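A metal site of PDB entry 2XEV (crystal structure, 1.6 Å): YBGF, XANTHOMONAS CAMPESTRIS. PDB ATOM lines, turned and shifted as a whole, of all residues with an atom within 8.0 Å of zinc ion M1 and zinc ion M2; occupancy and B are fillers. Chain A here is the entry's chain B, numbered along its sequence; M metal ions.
The side-chain carboxylate (OE2) of Glu 59 lies close to the side-chain amide nitrogen (NE2) of Gln 86. OE2 of Glu 59 sits close to NH2 of Arg 63, at 3.4 Å. The backbone carbonyl oxygen (O) of Glu 94 sits close to the side-chain amide oxygen (OE1) of Gln 86, 3.4 Å away. The side-chain carboxylate (OE2) of Glu 94 is in salt-bridge range of the guanidinium group (NH2) of Arg 63, at 3.8 Å. The backbone carbonyl oxygen (O) of Glu 94 lies within hydrogen-bond range of the side-chain hydroxyl (OG1) of Thr 98 (3.1 Å). N of Lys 91 is in hydrogen-bond range of O of Gln 86 (3.0 Å). The guanidinium group (NH2) of Arg 63 sits close to the side-chain amide nitrogen (NE2) of Gln 86, at 3.3 Å. OE1 of Gln 86 is in hydrogen-bond range of OG1 of Thr 98, 2.6 Å away.
Gln 86 touches zinc ion M1. Lys 91 touches zinc ion M1. Within 4 Å of zinc ion M1: Glu 59, Gln 86, Glu 89, Lys 91 and Glu 94.
NZ of Lys 91 touches zinc ion M2, 3.8 Å away. Three residues have an atom within 4 Å of zinc ion M2: Glu 59, Glu 89 and Lys 91. The nearest printed residue that does not touch zinc ion M2 is Gln 56 (4.3 Å).
Zinc ion M1 is bound by the side-chain carboxylate of Glu 89 (1.9 Å), the side-chain carboxylate of Glu 59 (2.1 Å) and the side-chain carboxylate of Glu 94 (2.1 Å).
Zinc ion M2 is bound by the side-chain carboxylate of Glu 89 (1.9 Å) and the side-chain carboxylate of Glu 59 (2.1 Å).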
ATOM      1  N   PHE A  55      29.315  -8.085 -21.635  1.00  0.00           N
ATOM      2  CA  PHE A  55      29.319  -9.156 -20.631  1.00  0.00           C
ATOM      3  C   PHE A  55      29.823 -10.509 -21.153  1.00  0.00           C
ATOM      4  O   PHE A  55      30.413 -11.274 -20.378  1.00  0.00           O
ATOM      5  CB  PHE A  55      27.956  -9.284 -19.957  1.00  0.00           C
ATOM      6  CG  PHE A  55      27.521  -8.024 -19.255  1.00  0.00           C
ATOM      7  CD1 PHE A  55      28.238  -7.551 -18.154  1.00  0.00           C
ATOM      8  CD2 PHE A  55      26.405  -7.317 -19.708  1.00  0.00           C
ATOM      9  CE1 PHE A  55      27.850  -6.365 -17.512  1.00  0.00           C
ATOM     10  CE2 PHE A  55      26.007  -6.122 -19.064  1.00  0.00           C
ATOM     11  CZ  PHE A  55      26.723  -5.650 -17.963  1.00  0.00           C
ATOM     12  N   GLN A  56      29.585 -10.795 -22.433  1.00  0.00           N
ATOM     13  CA  GLN A  56      30.026 -12.076 -23.016  1.00  0.00           C
ATOM     14  C   GLN A  56      31.550 -12.094 -23.156  1.00  0.00           C
ATOM     15  O   GLN A  56      32.214 -13.091 -22.821  1.00  0.00           O
ATOM     16  CB  GLN A  56      29.362 -12.320 -24.371  1.00  0.00           C
ATOM     17  CG  GLN A  56      27.862 -12.429 -24.268  1.00  0.00           C
ATOM     18  CD  GLN A  56      27.209 -12.470 -25.626  1.00  0.00           C
ATOM     19  OE1 GLN A  56      26.834 -11.424 -26.177  1.00  0.00           O
ATOM     20  NE2 GLN A  56      27.109 -13.657 -26.190  1.00  0.00           N
ATOM     21  N   LEU A  57      32.102 -10.969 -23.609  1.00  0.00           N
ATOM     22  CA  LEU A  57      33.542 -10.841 -23.722  1.00  0.00           C
ATOM     23  C   LEU A  57      34.172 -10.894 -22.332  1.00  0.00           C
ATOM     24  O   LEU A  57      35.196 -11.562 -22.132  1.00  0.00           O
ATOM     25  CB  LEU A  57      33.951  -9.553 -24.456  1.00  0.00           C
ATOM     26  CG  LEU A  57      33.464  -9.428 -25.907  1.00  0.00           C
ATOM     27  CD1 LEU A  57      33.958  -8.129 -26.513  1.00  0.00           C
ATOM     28  CD2 LEU A  57      33.965 -10.619 -26.746  1.00  0.00           C
ATOM     29  N   GLU A  59      32.886 -12.374 -19.577  1.00  0.00           N
ATOM     30  CA  GLU A  59      32.754 -13.765 -19.166  1.00  0.00           C
ATOM     31  C   GLU A  59      33.921 -14.630 -19.646  1.00  0.00           C
ATOM     32  O   GLU A  59      34.476 -15.404 -18.847  1.00  0.00           O
ATOM     33  CB  GLU A  59      31.436 -14.321 -19.725  1.00  0.00           C
ATOM     34  CG  GLU A  59      31.291 -15.839 -19.561  1.00  0.00           C
ATOM     35  CD  GLU A  59      29.947 -16.342 -20.057  1.00  0.00           C
ATOM     36  OE1 GLU A  59      29.603 -16.116 -21.240  1.00  0.00           O
ATOM     37  OE2 GLU A  59      29.251 -16.960 -19.232  1.00  0.00           O
ATOM     38  N   ALA A  60      34.286 -14.509 -20.921  1.00  0.00           N
ATOM     39  CA  ALA A  60      35.355 -15.334 -21.478  1.00  0.00           C
ATOM     40  C   ALA A  60      36.692 -15.110 -20.788  1.00  0.00           C
ATOM     41  O   ALA A  60      37.435 -16.073 -20.548  1.00  0.00           O
ATOM     42  CB  ALA A  60      35.478 -15.116 -22.987  1.00  0.00           C
ATOM     43  N   ARG A  63      36.514 -16.488 -17.103  1.00  0.00           N
ATOM     44  CA  ARG A  63      36.521 -17.951 -17.187  1.00  0.00           C
ATOM     45  C   ARG A  63      37.942 -18.446 -17.404  1.00  0.00           C
ATOM     46  O   ARG A  63      38.369 -19.384 -16.742  1.00  0.00           O
ATOM     47  CB  ARG A  63      35.608 -18.411 -18.328  1.00  0.00           C
ATOM     48  CG  ARG A  63      35.587 -19.929 -18.606  1.00  0.00           C
ATOM     49  CD  ARG A  63      34.414 -20.229 -19.576  1.00  0.00           C
ATOM     50  NE  ARG A  63      33.144 -20.212 -18.842  1.00  0.00           N
ATOM     51  CZ  ARG A  63      31.965 -19.794 -19.320  1.00  0.00           C
ATOM     52  NH1 ARG A  63      31.844 -19.325 -20.551  1.00  0.00           N
ATOM     53  NH2 ARG A  63      30.900 -19.836 -18.526  1.00  0.00           N
ATOM     54  N   LEU A  82      33.010 -13.189 -12.894  1.00  0.00           N
ATOM     55  CA  LEU A  82      32.416 -14.106 -13.844  1.00  0.00           C
ATOM     56  C   LEU A  82      30.912 -14.190 -13.584  1.00  0.00           C
ATOM     57  O   LEU A  82      30.109 -13.964 -14.482  1.00  0.00           O
ATOM     58  CB  LEU A  82      33.071 -15.480 -13.768  1.00  0.00           C
ATOM     59  CG  LEU A  82      32.489 -16.578 -14.684  1.00  0.00           C
ATOM     60  CD1 LEU A  82      32.457 -16.122 -16.146  1.00  0.00           C
ATOM     61  CD2 LEU A  82      33.247 -17.911 -14.529  1.00  0.00           C
ATOM     62  N   GLY A  83      30.552 -14.493 -12.338  1.00  0.00           N
ATOM     63  CA  GLY A  83      29.130 -14.551 -11.940  1.00  0.00           C
ATOM     64  C   GLY A  83      28.387 -13.264 -12.252  1.00  0.00           C
ATOM     65  O   GLY A  83      27.268 -13.298 -12.761  1.00  0.00           O
ATOM     66  N   SER A  85      29.160 -11.009 -14.500  1.00  0.00           N
ATOM     67  CA  SER A  85      29.063 -10.895 -15.959  1.00  0.00           C
ATOM     68  C   SER A  85      27.910 -11.760 -16.501  1.00  0.00           C
ATOM     69  O   SER A  85      27.186 -11.342 -17.384  1.00  0.00           O
ATOM     70  CB  SER A  85      30.376 -11.334 -16.601  1.00  0.00           C
ATOM     71  OG  SER A  85      31.428 -10.468 -16.207  1.00  0.00           O
ATOM     72  N   GLN A  86      27.761 -12.965 -15.953  1.00  0.00           N
ATOM     73  CA  GLN A  86      26.663 -13.844 -16.316  1.00  0.00           C
ATOM     74  C   GLN A  86      25.308 -13.226 -15.951  1.00  0.00           C
ATOM     75  O   GLN A  86      24.353 -13.260 -16.752  1.00  0.00           O
ATOM     76  CB  GLN A  86      26.883 -15.244 -15.727  1.00  0.00           C
ATOM     77  CG  GLN A  86      28.190 -15.886 -16.246  1.00  0.00           C
ATOM     78  CD  GLN A  86      28.589 -17.163 -15.514  1.00  0.00           C
ATOM     79  OE1 GLN A  86      28.288 -17.332 -14.339  1.00  0.00           O
ATOM     80  NE2 GLN A  86      29.302 -18.059 -16.214  1.00  0.00           N
ATOM     81  N   TYR A  87      25.235 -12.574 -14.787  1.00  0.00           N
ATOM     82  CA  TYR A  87      24.028 -11.834 -14.427  1.00  0.00           C
ATOM     83  C   TYR A  87      23.768 -10.720 -15.438  1.00  0.00           C
ATOM     84  O   TYR A  87      22.621 -10.478 -15.829  1.00  0.00           O
ATOM     85  CB  TYR A  87      24.129 -11.299 -12.994  1.00  0.00           C
ATOM     86  CG  TYR A  87      22.867 -10.576 -12.560  1.00  0.00           C
ATOM     87  CD1 TYR A  87      21.707 -11.286 -12.233  1.00  0.00           C
ATOM     88  CD2 TYR A  87      22.828  -9.199 -12.499  1.00  0.00           C
ATOM     89  CE1 TYR A  87      20.545 -10.599 -11.827  1.00  0.00           C
ATOM     90  CE2 TYR A  87      21.678  -8.515 -12.104  1.00  0.00           C
ATOM     91  CZ  TYR A  87      20.549  -9.218 -11.780  1.00  0.00           C
ATOM     92  OH  TYR A  87      19.419  -8.520 -11.385  1.00  0.00           O
ATOM     93  N   GLU A  89      24.562 -10.855 -18.544  1.00  0.00           N
ATOM     94  CA  GLU A  89      24.108 -11.576 -19.764  1.00  0.00           C
ATOM     95  C   GLU A  89      22.616 -11.900 -19.651  1.00  0.00           C
ATOM     96  O   GLU A  89      22.003 -12.354 -20.615  1.00  0.00           O
ATOM     97  CB  GLU A  89      24.820 -12.921 -19.921  1.00  0.00           C
ATOM     98  CG  GLU A  89      26.276 -12.920 -20.372  1.00  0.00           C
ATOM     99  CD  GLU A  89      26.780 -14.355 -20.635  1.00  0.00           C
ATOM    100  OE1 GLU A  89      26.769 -15.197 -19.707  1.00  0.00           O
ATOM    101  OE2 GLU A  89      27.154 -14.673 -21.800  1.00  0.00           O
ATOM    102  N   GLY A  90      22.048 -11.678 -18.462  1.00  0.00           N
ATOM    103  CA  GLY A  90      20.667 -12.084 -18.177  1.00  0.00           C
ATOM    104  C   GLY A  90      20.537 -13.558 -17.805  1.00  0.00           C
ATOM    105  O   GLY A  90      19.420 -14.075 -17.673  1.00  0.00           O
ATOM    106  N   LYS A  91      21.668 -14.231 -17.625  1.00  0.00           N
ATOM    107  CA  LYS A  91      21.686 -15.647 -17.286  1.00  0.00           C
ATOM    108  C   LYS A  91      21.704 -15.843 -15.773  1.00  0.00           C
ATOM    109  O   LYS A  91      22.745 -16.164 -15.201  1.00  0.00           O
ATOM    110  CB  LYS A  91      22.865 -16.363 -17.957  1.00  0.00           C
ATOM    111  CG  LYS A  91      22.822 -16.249 -19.477  1.00  0.00           C
ATOM    112  CD  LYS A  91      23.705 -17.255 -20.179  1.00  0.00           C
ATOM    113  CE  LYS A  91      23.426 -17.231 -21.678  1.00  0.00           C
ATOM    114  NZ  LYS A  91      24.444 -18.012 -22.443  1.00  0.00           N
ATOM    115  N   GLU A  94      22.854 -19.400 -14.294  1.00  0.00           N
ATOM    116  CA  GLU A  94      24.298 -19.533 -14.461  1.00  0.00           C
ATOM    117  C   GLU A  94      24.989 -18.662 -13.427  1.00  0.00           C
ATOM    118  O   GLU A  94      25.923 -19.118 -12.756  1.00  0.00           O
ATOM    119  CB  GLU A  94      24.720 -19.119 -15.878  1.00  0.00           C
ATOM    120  CG  GLU A  94      26.107 -19.613 -16.326  1.00  0.00           C
ATOM    121  CD  GLU A  94      26.531 -19.054 -17.689  1.00  0.00           C
ATOM    122  OE1 GLU A  94      26.292 -17.864 -17.947  1.00  0.00           O
ATOM    123  OE2 GLU A  94      27.135 -19.806 -18.486  1.00  0.00           O
ATOM    124  N   ALA A  95      24.530 -17.417 -13.286  1.00  0.00           N
ATOM    125  CA  ALA A  95      25.145 -16.466 -12.347  1.00  0.00           C
ATOM    126  C   ALA A  95      25.056 -16.938 -10.894  1.00  0.00           C
ATOM    127  O   ALA A  95      26.030 -16.859 -10.145  1.00  0.00           O
ATOM    128  CB  ALA A  95      24.555 -15.079 -12.487  1.00  0.00           C
ATOM    129  N   THR A  98      27.543 -19.724 -10.255  1.00  0.00           N
ATOM    130  CA  THR A  98      28.918 -19.218 -10.193  1.00  0.00           C
ATOM    131  C   THR A  98      29.205 -18.483  -8.864  1.00  0.00           C
ATOM    132  O   THR A  98      30.253 -18.672  -8.256  1.00  0.00           O
ATOM    133  CB  THR A  98      29.207 -18.322 -11.430  1.00  0.00           C
ATOM    134  OG1 THR A  98      29.067 -19.097 -12.626  1.00  0.00           O
ATOM    135  CG2 THR A  98      30.627 -17.728 -11.365  1.00  0.00           C
HETATM  136 ZN    ZN M   1      27.237 -17.053 -19.606  1.00  0.00          ZN
HETATM  137 ZN    ZN M   2      27.861 -16.333 -22.439  1.00  0.00          ZN
